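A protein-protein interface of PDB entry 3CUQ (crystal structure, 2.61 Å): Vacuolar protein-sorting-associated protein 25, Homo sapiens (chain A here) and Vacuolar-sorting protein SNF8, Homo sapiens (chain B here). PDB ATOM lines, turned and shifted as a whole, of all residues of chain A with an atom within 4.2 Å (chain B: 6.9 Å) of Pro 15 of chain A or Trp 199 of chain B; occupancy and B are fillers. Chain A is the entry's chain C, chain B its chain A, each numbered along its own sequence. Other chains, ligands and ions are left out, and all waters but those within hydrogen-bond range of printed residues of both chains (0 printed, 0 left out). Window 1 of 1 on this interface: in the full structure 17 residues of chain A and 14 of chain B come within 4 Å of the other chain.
Among the printed residues, merely in contact across the chains: Gln 20 of chain A with Trp 199 of chain B (3.3 Å), Pro 15 of chain A with Trp 199 of chain B (3.4 Å), Pro 15 of chain A with Leu 200 of chain B (3.5 Å), Phe 13 of chain A with Pro 213 of chain B (3.5 Å), Pro 15 of chain A with Trp 211 of chain B (3.5 Å), Thr 25 of chain A with Trp 199 of chain B (3.6 Å), Phe 13 of chain A with Trp 211 of chain B (3.6 Å), Phe 13 of chain A with Phe 216 of chain B (3.7 Å), Pro 14 of chain A with Asp 201 of chain B (3.7 Å), Pro 14 of chain A with Trp 211 of chain B (3.8 Å), Phe 13 of chain A with Trp 199 of chain B (3.8 Å), Thr 18 of chain A with Leu 200 of chain B (3.8 Å), Thr 18 of chain A with Gln 203 of chain B (3.9 Å) and Gln 29 of chain A with Trp 199 of chain B (3.997 Å).
Of the 9 printed residues of chain A, 8 touch a printed residue of chain B.
Hydrophobic or aromatic side chains of chain A that line the printed part of chain B: Phe 13, Pro 14 and Pro 15.
Printed residues of chain B that touch a printed residue of chain A: Trp 199, Leu 200, Asp 201, Leu 202, Gln 203, Trp 211, Pro 213 and Phe 216.
Hydrophobic or aromatic side chains of chain B within 4 Å of the printed part of chain A: Trp 199, Leu 200, Leu 202, Trp 211, Pro 213 and Phe 216.
Among the printed residues, 17 pairs touch across the chains.
Among the printed residues, no Asp or Glu carboxylate lies within 4 Å of a Lys or Arg side-chain nitrogen of the other chain.
The side-chain amide nitrogen (NE2) of Gln 20 of chain A sits at hydrogen-bond distance from the backbone carbonyl oxygen (O) of Leu 200 of chain B (2.7 Å).
The backbone NH of Leu 202 of chain B is in hydrogen-bond range of the side-chain hydroxyl of Thr 18 of chain A (3.2 Å).
NE2 of Gln 203 of chain B sits at hydrogen-bond distance from O of Phe 17 of chain A, 2.9 Å away.
Of chain B, only Trp 199, Leu 200 and Trp 211 come within 4 Å of Pro 15 of chain A.
Of the printed residues of chain A, Trp 199 of chain B touches Phe 13, Pro 15, Gln 20, Thr 25 and Gln 29.
Of the printed residues of chain A, Gln 203 of chain B touches Phe 17 (2.9 Å) and Thr 18 (3.9 Å).
Of the printed residues of chain B, Phe 17 of chain A touches Gln 203.
Printed residues of chain A within 4 Å of Phe 216 of chain B: Phe 13 (3.7 Å).
Arg 90 of chain B touches none of the printed residues of chain A.
Phe 16 of chain A touches none of the printed residues of chain B.
The nearest residue of chain B that does not touch Pro 15 of chain A is Asp 201 of chain B (4.1 Å).
The backbone carbonyl oxygen of Trp 211 of chain B sits at hydrogen-bond distance from the backbone NH of Trp 199 of chain B (2.9 Å).
OD2 of Asp 201 of chain B lies within hydrogen-bond range of N of Gln 203 of chain B (2.8 Å).
OD1 of Asp 201 of chain B sits at hydrogen-bond distance from NE1 of Trp 211 of chain B.
O of Pro 15 of chain A sits at hydrogen-bond distance from NE2 of Gln 20 of chain A (3.3 Å).
O of Thr 18 of chain A sits at hydrogen-bond distance from NE2 of Gln 20 of chain A.
The backbone carbonyl oxygen (O) of Thr 18 of chain A lies within hydrogen-bond range of the side-chain amide nitrogen (NE2) of Gln 29 of chain A.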
ATOM      1  N   PHE A  13     -32.627 -26.092  -2.003  1.00  0.00           N
ATOM      2  CA  PHE A  13     -31.619 -25.162  -1.499  1.00  0.00           C
ATOM      3  C   PHE A  13     -31.933 -23.798  -2.085  1.00  0.00           C
ATOM      4  O   PHE A  13     -31.726 -23.594  -3.263  1.00  0.00           O
ATOM      5  CB  PHE A  13     -30.241 -25.632  -2.044  1.00  0.00           C
ATOM      6  CG  PHE A  13     -29.044 -24.936  -1.418  1.00  0.00           C
ATOM      7  CD1 PHE A  13     -28.931 -24.821   0.004  1.00  0.00           C
ATOM      8  CD2 PHE A  13     -28.018 -24.414  -2.229  1.00  0.00           C
ATOM      9  CE1 PHE A  13     -27.805 -24.218   0.591  1.00  0.00           C
ATOM     10  CE2 PHE A  13     -26.865 -23.782  -1.631  1.00  0.00           C
ATOM     11  CZ  PHE A  13     -26.770 -23.683  -0.211  1.00  0.00           C
ATOM     12  N   PRO A  14     -32.391 -22.845  -1.269  1.00  0.00           N
ATOM     13  CA  PRO A  14     -32.769 -21.510  -1.795  1.00  0.00           C
ATOM     14  C   PRO A  14     -31.899 -20.911  -2.898  1.00  0.00           C
ATOM     15  O   PRO A  14     -32.423 -20.456  -3.903  1.00  0.00           O
ATOM     16  CB  PRO A  14     -32.721 -20.632  -0.551  1.00  0.00           C
ATOM     17  CG  PRO A  14     -33.244 -21.577   0.520  1.00  0.00           C
ATOM     18  CD  PRO A  14     -32.640 -22.941   0.177  1.00  0.00           C
ATOM     19  N   PRO A  15     -30.566 -20.849  -2.699  1.00  0.00           N
ATOM     20  CA  PRO A  15     -29.674 -20.256  -3.695  1.00  0.00           C
ATOM     21  C   PRO A  15     -29.819 -20.823  -5.093  1.00  0.00           C
ATOM     22  O   PRO A  15     -29.531 -20.113  -6.073  1.00  0.00           O
ATOM     23  CB  PRO A  15     -28.313 -20.630  -3.163  1.00  0.00           C
ATOM     24  CG  PRO A  15     -28.504 -20.581  -1.684  1.00  0.00           C
ATOM     25  CD  PRO A  15     -29.819 -21.228  -1.468  1.00  0.00           C
ATOM     26  N   PHE A  16     -30.250 -22.083  -5.201  1.00  0.00           N
ATOM     27  CA  PHE A  16     -30.257 -22.791  -6.517  1.00  0.00           C
ATOM     28  C   PHE A  16     -31.020 -21.972  -7.523  1.00  0.00           C
ATOM     29  O   PHE A  16     -30.747 -22.024  -8.716  1.00  0.00           O
ATOM     30  CB  PHE A  16     -30.909 -24.167  -6.414  1.00  0.00           C
ATOM     31  CG  PHE A  16     -30.823 -24.971  -7.678  1.00  0.00           C
ATOM     32  CD1 PHE A  16     -29.605 -25.192  -8.294  1.00  0.00           C
ATOM     33  CD2 PHE A  16     -31.969 -25.539  -8.239  1.00  0.00           C
ATOM     34  CE1 PHE A  16     -29.538 -25.949  -9.439  1.00  0.00           C
ATOM     35  CE2 PHE A  16     -31.921 -26.290  -9.355  1.00  0.00           C
ATOM     36  CZ  PHE A  16     -30.702 -26.497  -9.969  1.00  0.00           C
ATOM     37  N   PHE A  17     -31.965 -21.207  -6.969  1.00  0.00           N
ATOM     38  CA  PHE A  17     -32.908 -20.376  -7.695  1.00  0.00           C
ATOM     39  C   PHE A  17     -32.390 -18.983  -8.086  1.00  0.00           C
ATOM     40  O   PHE A  17     -33.165 -18.176  -8.587  1.00  0.00           O
ATOM     41  CB  PHE A  17     -34.237 -20.309  -6.919  1.00  0.00           C
ATOM     42  CG  PHE A  17     -34.923 -21.661  -6.799  1.00  0.00           C
ATOM     43  CD1 PHE A  17     -34.654 -22.513  -5.722  1.00  0.00           C
ATOM     44  CD2 PHE A  17     -35.805 -22.110  -7.785  1.00  0.00           C
ATOM     45  CE1 PHE A  17     -35.269 -23.784  -5.614  1.00  0.00           C
ATOM     46  CE2 PHE A  17     -36.417 -23.380  -7.689  1.00  0.00           C
ATOM     47  CZ  PHE A  17     -36.146 -24.218  -6.601  1.00  0.00           C
ATOM     48  N   THR A  18     -31.108 -18.700  -7.841  1.00  0.00           N
ATOM     49  CA  THR A  18     -30.464 -17.445  -8.279  1.00  0.00           C
ATOM     50  C   THR A  18     -29.235 -17.690  -9.171  1.00  0.00           C
ATOM     51  O   THR A  18     -28.386 -18.516  -8.841  1.00  0.00           O
ATOM     52  CB  THR A  18     -29.949 -16.623  -7.095  1.00  0.00           C
ATOM     53  OG1 THR A  18     -31.030 -15.989  -6.419  1.00  0.00           O
ATOM     54  CG2 THR A  18     -29.004 -15.542  -7.607  1.00  0.00           C
ATOM     55  N   GLN A  20     -25.846 -17.715 -10.107  1.00  0.00           N
ATOM     56  CA  GLN A  20     -24.755 -17.502  -9.191  1.00  0.00           C
ATOM     57  C   GLN A  20     -23.692 -16.722  -9.928  1.00  0.00           C
ATOM     58  O   GLN A  20     -23.410 -17.018 -11.092  1.00  0.00           O
ATOM     59  CB  GLN A  20     -24.215 -18.825  -8.720  1.00  0.00           C
ATOM     60  CG  GLN A  20     -25.143 -19.578  -7.860  1.00  0.00           C
ATOM     61  CD  GLN A  20     -25.336 -18.888  -6.552  1.00  0.00           C
ATOM     62  OE1 GLN A  20     -24.356 -18.487  -5.917  1.00  0.00           O
ATOM     63  NE2 GLN A  20     -26.588 -18.730  -6.122  1.00  0.00           N
ATOM     64  N   THR A  25     -19.166 -22.042  -9.691  1.00  0.00           N
ATOM     65  CA  THR A  25     -20.451 -22.398  -9.149  1.00  0.00           C
ATOM     66  C   THR A  25     -21.584 -22.339 -10.206  1.00  0.00           C
ATOM     67  O   THR A  25     -22.462 -23.161 -10.202  1.00  0.00           O
ATOM     68  CB  THR A  25     -20.753 -21.526  -7.962  1.00  0.00           C
ATOM     69  OG1 THR A  25     -19.661 -21.651  -7.061  1.00  0.00           O
ATOM     70  CG2 THR A  25     -21.935 -22.040  -7.155  1.00  0.00           C
ATOM     71  N   GLN A  29     -24.328 -25.040 -11.130  1.00  0.00           N
ATOM     72  CA  GLN A  29     -25.724 -24.732 -11.010  1.00  0.00           C
ATOM     73  C   GLN A  29     -26.435 -25.197 -12.309  1.00  0.00           C
ATOM     74  O   GLN A  29     -27.447 -25.879 -12.248  1.00  0.00           O
ATOM     75  CB  GLN A  29     -25.875 -23.229 -10.818  1.00  0.00           C
ATOM     76  CG  GLN A  29     -27.267 -22.800 -10.470  1.00  0.00           C
ATOM     77  CD  GLN A  29     -27.390 -21.322 -10.264  1.00  0.00           C
ATOM     78  OE1 GLN A  29     -26.620 -20.537 -10.795  1.00  0.00           O
ATOM     79  NE2 GLN A  29     -28.355 -20.924  -9.455  1.00  0.00           N
ATOM     80  N   HIS B  89     -17.765 -31.638  -4.175  1.00  0.00           N
ATOM     81  CA  HIS B  89     -18.525 -30.931  -5.207  1.00  0.00           C
ATOM     82  C   HIS B  89     -19.843 -30.301  -4.718  1.00  0.00           C
ATOM     83  O   HIS B  89     -20.219 -29.227  -5.189  1.00  0.00           O
ATOM     84  CB  HIS B  89     -18.801 -31.840  -6.412  1.00  0.00           C
ATOM     85  CG  HIS B  89     -19.769 -32.947  -6.107  1.00  0.00           C
ATOM     86  ND1 HIS B  89     -20.914 -33.167  -6.849  1.00  0.00           N
ATOM     87  CD2 HIS B  89     -19.805 -33.840  -5.085  1.00  0.00           C
ATOM     88  CE1 HIS B  89     -21.584 -34.181  -6.326  1.00  0.00           C
ATOM     89  NE2 HIS B  89     -20.936 -34.604  -5.254  1.00  0.00           N
ATOM     90  N   ARG B  90     -20.565 -30.943  -3.806  1.00  0.00           N
ATOM     91  CA  ARG B  90     -21.747 -30.296  -3.261  1.00  0.00           C
ATOM     92  C   ARG B  90     -21.350 -29.119  -2.367  1.00  0.00           C
ATOM     93  O   ARG B  90     -21.903 -28.017  -2.444  1.00  0.00           O
ATOM     94  CB  ARG B  90     -22.577 -31.272  -2.426  1.00  0.00           C
ATOM     95  CG  ARG B  90     -23.074 -32.494  -3.161  1.00  0.00           C
ATOM     96  CD  ARG B  90     -23.193 -33.634  -2.167  1.00  0.00           C
ATOM     97  NE  ARG B  90     -24.357 -34.489  -2.401  1.00  0.00           N
ATOM     98  CZ  ARG B  90     -24.453 -35.373  -3.387  1.00  0.00           C
ATOM     99  NH1 ARG B  90     -23.471 -35.527  -4.271  1.00  0.00           N
ATOM    100  NH2 ARG B  90     -25.544 -36.103  -3.499  1.00  0.00           N
ATOM    101  N   ASN B  91     -20.386 -29.361  -1.504  1.00  0.00           N
ATOM    102  CA  ASN B  91     -20.191 -28.492  -0.385  1.00  0.00           C
ATOM    103  C   ASN B  91     -18.885 -27.684  -0.343  1.00  0.00           C
ATOM    104  O   ASN B  91     -18.690 -26.954   0.565  1.00  0.00           O
ATOM    105  CB  ASN B  91     -20.379 -29.312   0.883  1.00  0.00           C
ATOM    106  CG  ASN B  91     -19.235 -30.291   1.151  1.00  0.00           C
ATOM    107  OD1 ASN B  91     -18.106 -30.123   0.685  1.00  0.00           O
ATOM    108  ND2 ASN B  91     -19.523 -31.297   1.992  1.00  0.00           N
ATOM    109  N   LEU B 192     -15.929 -16.666   0.389  1.00  0.00           N
ATOM    110  CA  LEU B 192     -16.862 -17.741   0.466  1.00  0.00           C
ATOM    111  C   LEU B 192     -17.447 -18.090  -0.943  1.00  0.00           C
ATOM    112  O   LEU B 192     -17.335 -19.255  -1.402  1.00  0.00           O
ATOM    113  CB  LEU B 192     -17.914 -17.343   1.489  1.00  0.00           C
ATOM    114  CG  LEU B 192     -17.481 -17.343   2.973  1.00  0.00           C
ATOM    115  CD1 LEU B 192     -18.701 -17.206   3.938  1.00  0.00           C
ATOM    116  CD2 LEU B 192     -16.593 -18.542   3.408  1.00  0.00           C
ATOM    117  N   LEU B 193     -17.988 -17.098  -1.664  1.00  0.00           N
ATOM    118  CA  LEU B 193     -18.288 -17.332  -3.078  1.00  0.00           C
ATOM    119  C   LEU B 193     -17.104 -17.832  -3.894  1.00  0.00           C
ATOM    120  O   LEU B 193     -17.234 -18.860  -4.545  1.00  0.00           O
ATOM    121  CB  LEU B 193     -18.999 -16.151  -3.764  1.00  0.00           C
ATOM    122  CG  LEU B 193     -20.272 -15.717  -3.003  1.00  0.00           C
ATOM    123  CD1 LEU B 193     -20.904 -14.438  -3.558  1.00  0.00           C
ATOM    124  CD2 LEU B 193     -21.318 -16.837  -2.923  1.00  0.00           C
ATOM    125  N   GLY B 196     -16.444 -21.566  -3.474  1.00  0.00           N
ATOM    126  CA  GLY B 196     -17.529 -22.505  -3.543  1.00  0.00           C
ATOM    127  C   GLY B 196     -18.116 -22.874  -2.196  1.00  0.00           C
ATOM    128  O   GLY B 196     -18.776 -23.897  -2.086  1.00  0.00           O
ATOM    129  N   LEU B 197     -17.917 -22.082  -1.146  1.00  0.00           N
ATOM    130  CA  LEU B 197     -18.407 -22.530   0.129  1.00  0.00           C
ATOM    131  C   LEU B 197     -19.716 -21.894   0.402  1.00  0.00           C
ATOM    132  O   LEU B 197     -20.423 -22.286   1.343  1.00  0.00           O
ATOM    133  CB  LEU B 197     -17.433 -22.205   1.255  1.00  0.00           C
ATOM    134  CG  LEU B 197     -16.120 -22.974   1.206  1.00  0.00           C
ATOM    135  CD1 LEU B 197     -15.209 -22.453   2.305  1.00  0.00           C
ATOM    136  CD2 LEU B 197     -16.313 -24.446   1.366  1.00  0.00           C
ATOM    137  N   ALA B 198     -20.034 -20.867  -0.369  1.00  0.00           N
ATOM    138  CA  ALA B 198     -21.317 -20.199  -0.170  1.00  0.00           C
ATOM    139  C   ALA B 198     -21.942 -19.992  -1.530  1.00  0.00           C
ATOM    140  O   ALA B 198     -21.231 -20.001  -2.525  1.00  0.00           O
ATOM    141  CB  ALA B 198     -21.148 -18.902   0.572  1.00  0.00           C
ATOM    142  N   TRP B 199     -23.276 -19.906  -1.576  1.00  0.00           N
ATOM    143  CA  TRP B 199     -23.996 -19.539  -2.825  1.00  0.00           C
ATOM    144  C   TRP B 199     -24.872 -18.366  -2.410  1.00  0.00           C
ATOM    145  O   TRP B 199     -25.299 -18.266  -1.253  1.00  0.00           O
ATOM    146  CB  TRP B 199     -24.931 -20.624  -3.334  1.00  0.00           C
ATOM    147  CG  TRP B 199     -24.370 -21.905  -3.799  1.00  0.00           C
ATOM    148  CD1 TRP B 199     -23.336 -22.587  -3.273  1.00  0.00           C
ATOM    149  CD2 TRP B 199     -24.881 -22.714  -4.874  1.00  0.00           C
ATOM    150  NE1 TRP B 199     -23.140 -23.765  -3.974  1.00  0.00           N
ATOM    151  CE2 TRP B 199     -24.102 -23.870  -4.938  1.00  0.00           C
ATOM    152  CE3 TRP B 199     -25.933 -22.567  -5.775  1.00  0.00           C
ATOM    153  CZ2 TRP B 199     -24.326 -24.878  -5.885  1.00  0.00           C
ATOM    154  CZ3 TRP B 199     -26.153 -23.566  -6.709  1.00  0.00           C
ATOM    155  CH2 TRP B 199     -25.344 -24.698  -6.760  1.00  0.00           C
ATOM    156  N   LEU B 200     -25.142 -17.490  -3.374  1.00  0.00           N
ATOM    157  CA  LEU B 200     -25.861 -16.237  -3.108  1.00  0.00           C
ATOM    158  C   LEU B 200     -27.324 -16.500  -3.286  1.00  0.00           C
ATOM    159  O   LEU B 200     -27.698 -17.354  -4.097  1.00  0.00           O
ATOM    160  CB  LEU B 200     -25.408 -15.182  -4.117  1.00  0.00           C
ATOM    161  CG  LEU B 200     -25.994 -13.771  -4.035  1.00  0.00           C
ATOM    162  CD1 LEU B 200     -25.734 -13.053  -2.691  1.00  0.00           C
ATOM    163  CD2 LEU B 200     -25.478 -12.950  -5.270  1.00  0.00           C
ATOM    164  N   ASP B 201     -28.155 -15.749  -2.573  1.00  0.00           N
ATOM    165  CA  ASP B 201     -29.608 -15.901  -2.648  1.00  0.00           C
ATOM    166  C   ASP B 201     -30.252 -14.537  -2.646  1.00  0.00           C
ATOM    167  O   ASP B 201     -30.298 -13.866  -1.610  1.00  0.00           O
ATOM    168  CB  ASP B 201     -30.092 -16.773  -1.490  1.00  0.00           C
ATOM    169  CG  ASP B 201     -31.577 -16.624  -1.175  1.00  0.00           C
ATOM    170  OD1 ASP B 201     -31.968 -17.022  -0.057  1.00  0.00           O
ATOM    171  OD2 ASP B 201     -32.360 -16.120  -1.991  1.00  0.00           O
ATOM    172  N   LEU B 202     -30.744 -14.132  -3.818  1.00  0.00           N
ATOM    173  CA  LEU B 202     -31.342 -12.805  -3.997  1.00  0.00           C
ATOM    174  C   LEU B 202     -32.862 -12.755  -3.830  1.00  0.00           C
ATOM    175  O   LEU B 202     -33.491 -11.779  -4.258  1.00  0.00           O
ATOM    176  CB  LEU B 202     -30.951 -12.197  -5.333  1.00  0.00           C
ATOM    177  CG  LEU B 202     -29.470 -11.861  -5.518  1.00  0.00           C
ATOM    178  CD1 LEU B 202     -29.129 -11.548  -6.977  1.00  0.00           C
ATOM    179  CD2 LEU B 202     -29.069 -10.722  -4.567  1.00  0.00           C
ATOM    180  N   GLN B 203     -33.441 -13.774  -3.186  1.00  0.00           N
ATOM    181  CA  GLN B 203     -34.895 -13.853  -2.975  1.00  0.00           C
ATOM    182  C   GLN B 203     -35.208 -14.067  -1.494  1.00  0.00           C
ATOM    183  O   GLN B 203     -36.202 -14.695  -1.112  1.00  0.00           O
ATOM    184  CB  GLN B 203     -35.497 -14.947  -3.849  1.00  0.00           C
ATOM    185  CG  GLN B 203     -35.329 -14.695  -5.373  1.00  0.00           C
ATOM    186  CD  GLN B 203     -35.687 -15.917  -6.208  1.00  0.00           C
ATOM    187  OE1 GLN B 203     -36.681 -16.583  -5.918  1.00  0.00           O
ATOM    188  NE2 GLN B 203     -34.867 -16.232  -7.239  1.00  0.00           N
ATOM    189  N   HIS B 209     -28.797 -13.210   1.189  1.00  0.00           N
ATOM    190  CA  HIS B 209     -28.312 -14.180   2.180  1.00  0.00           C
ATOM    191  C   HIS B 209     -27.230 -14.968   1.464  1.00  0.00           C
ATOM    192  O   HIS B 209     -27.268 -15.074   0.228  1.00  0.00           O
ATOM    193  CB  HIS B 209     -29.402 -15.168   2.526  1.00  0.00           C
ATOM    194  CG  HIS B 209     -30.458 -14.614   3.416  1.00  0.00           C
ATOM    195  ND1 HIS B 209     -30.974 -13.347   3.258  1.00  0.00           N
ATOM    196  CD2 HIS B 209     -31.111 -15.163   4.467  1.00  0.00           C
ATOM    197  CE1 HIS B 209     -31.875 -13.126   4.199  1.00  0.00           C
ATOM    198  NE2 HIS B 209     -31.965 -14.208   4.953  1.00  0.00           N
ATOM    199  N   TYR B 210     -26.277 -15.507   2.233  1.00  0.00           N
ATOM    200  CA  TYR B 210     -25.188 -16.311   1.683  1.00  0.00           C
ATOM    201  C   TYR B 210     -25.263 -17.637   2.402  1.00  0.00           C
ATOM    202  O   TYR B 210     -25.025 -17.702   3.600  1.00  0.00           O
ATOM    203  CB  TYR B 210     -23.852 -15.641   1.934  1.00  0.00           C
ATOM    204  CG  TYR B 210     -23.696 -14.339   1.198  1.00  0.00           C
ATOM    205  CD1 TYR B 210     -24.402 -13.203   1.581  1.00  0.00           C
ATOM    206  CD2 TYR B 210     -22.851 -14.237   0.156  1.00  0.00           C
ATOM    207  CE1 TYR B 210     -24.261 -12.018   0.906  1.00  0.00           C
ATOM    208  CE2 TYR B 210     -22.714 -13.076  -0.528  1.00  0.00           C
ATOM    209  CZ  TYR B 210     -23.407 -11.968  -0.148  1.00  0.00           C
ATOM    210  OH  TYR B 210     -23.240 -10.801  -0.853  1.00  0.00           O
ATOM    211  N   TRP B 211     -25.691 -18.670   1.695  1.00  0.00           N
ATOM    212  CA  TRP B 211     -25.955 -19.976   2.277  1.00  0.00           C
ATOM    213  C   TRP B 211     -24.800 -20.932   2.005  1.00  0.00           C
ATOM    214  O   TRP B 211     -24.319 -21.026   0.852  1.00  0.00           O
ATOM    215  CB  TRP B 211     -27.197 -20.585   1.630  1.00  0.00           C
ATOM    216  CG  TRP B 211     -28.450 -19.865   1.850  1.00  0.00           C
ATOM    217  CD1 TRP B 211     -28.833 -18.692   1.264  1.00  0.00           C
ATOM    218  CD2 TRP B 211     -29.557 -20.296   2.658  1.00  0.00           C
ATOM    219  NE1 TRP B 211     -30.100 -18.331   1.711  1.00  0.00           N
ATOM    220  CE2 TRP B 211     -30.562 -19.304   2.560  1.00  0.00           C
ATOM    221  CE3 TRP B 211     -29.776 -21.397   3.487  1.00  0.00           C
ATOM    222  CZ2 TRP B 211     -31.772 -19.398   3.232  1.00  0.00           C
ATOM    223  CZ3 TRP B 211     -30.957 -21.475   4.199  1.00  0.00           C
ATOM    224  CH2 TRP B 211     -31.955 -20.478   4.066  1.00  0.00           C
ATOM    225  N   LEU B 212     -24.383 -21.659   3.032  1.00  0.00           N
ATOM    226  CA  LEU B 212     -23.347 -22.674   2.870  1.00  0.00           C
ATOM    227  C   LEU B 212     -23.885 -24.112   2.802  1.00  0.00           C
ATOM    228  O   LEU B 212     -24.268 -24.701   3.845  1.00  0.00           O
ATOM    229  CB  LEU B 212     -22.330 -22.581   4.023  1.00  0.00           C
ATOM    230  CG  LEU B 212     -21.568 -21.277   4.352  1.00  0.00           C
ATOM    231  CD1 LEU B 212     -22.393 -20.345   5.221  1.00  0.00           C
ATOM    232  CD2 LEU B 212     -20.167 -21.519   5.015  1.00  0.00           C
ATOM    233  N   PRO B 213     -23.844 -24.721   1.614  1.00  0.00           N
ATOM    234  CA  PRO B 213     -24.184 -26.136   1.414  1.00  0.00           C
ATOM    235  C   PRO B 213     -23.584 -27.070   2.463  1.00  0.00           C
ATOM    236  O   PRO B 213     -24.211 -28.077   2.819  1.00  0.00           O
ATOM    237  CB  PRO B 213     -23.605 -26.479   0.049  1.00  0.00           C
ATOM    238  CG  PRO B 213     -23.153 -25.186  -0.580  1.00  0.00           C
ATOM    239  CD  PRO B 213     -23.377 -24.055   0.390  1.00  0.00           C
ATOM    240  N   PHE B 216     -26.894 -26.936   6.137  1.00  0.00           N
ATOM    241  CA  PHE B 216     -27.972 -27.354   5.230  1.00  0.00           C
ATOM    242  C   PHE B 216     -28.143 -28.870   5.101  1.00  0.00           C
ATOM    243  O   PHE B 216     -27.470 -29.556   4.312  1.00  0.00           O
ATOM    244  CB  PHE B 216     -27.879 -26.741   3.824  1.00  0.00           C
ATOM    245  CG  PHE B 216     -29.142 -26.924   3.033  1.00  0.00           C
ATOM    246  CD1 PHE B 216     -30.269 -26.161   3.321  1.00  0.00           C
ATOM    247  CD2 PHE B 216     -29.229 -27.890   2.057  1.00  0.00           C
ATOM    248  CE1 PHE B 216     -31.441 -26.344   2.649  1.00  0.00           C
ATOM    249  CE2 PHE B 216     -30.413 -28.078   1.353  1.00  0.00           C
ATOM    250  CZ  PHE B 216     -31.522 -27.299   1.658  1.00  0.00           C
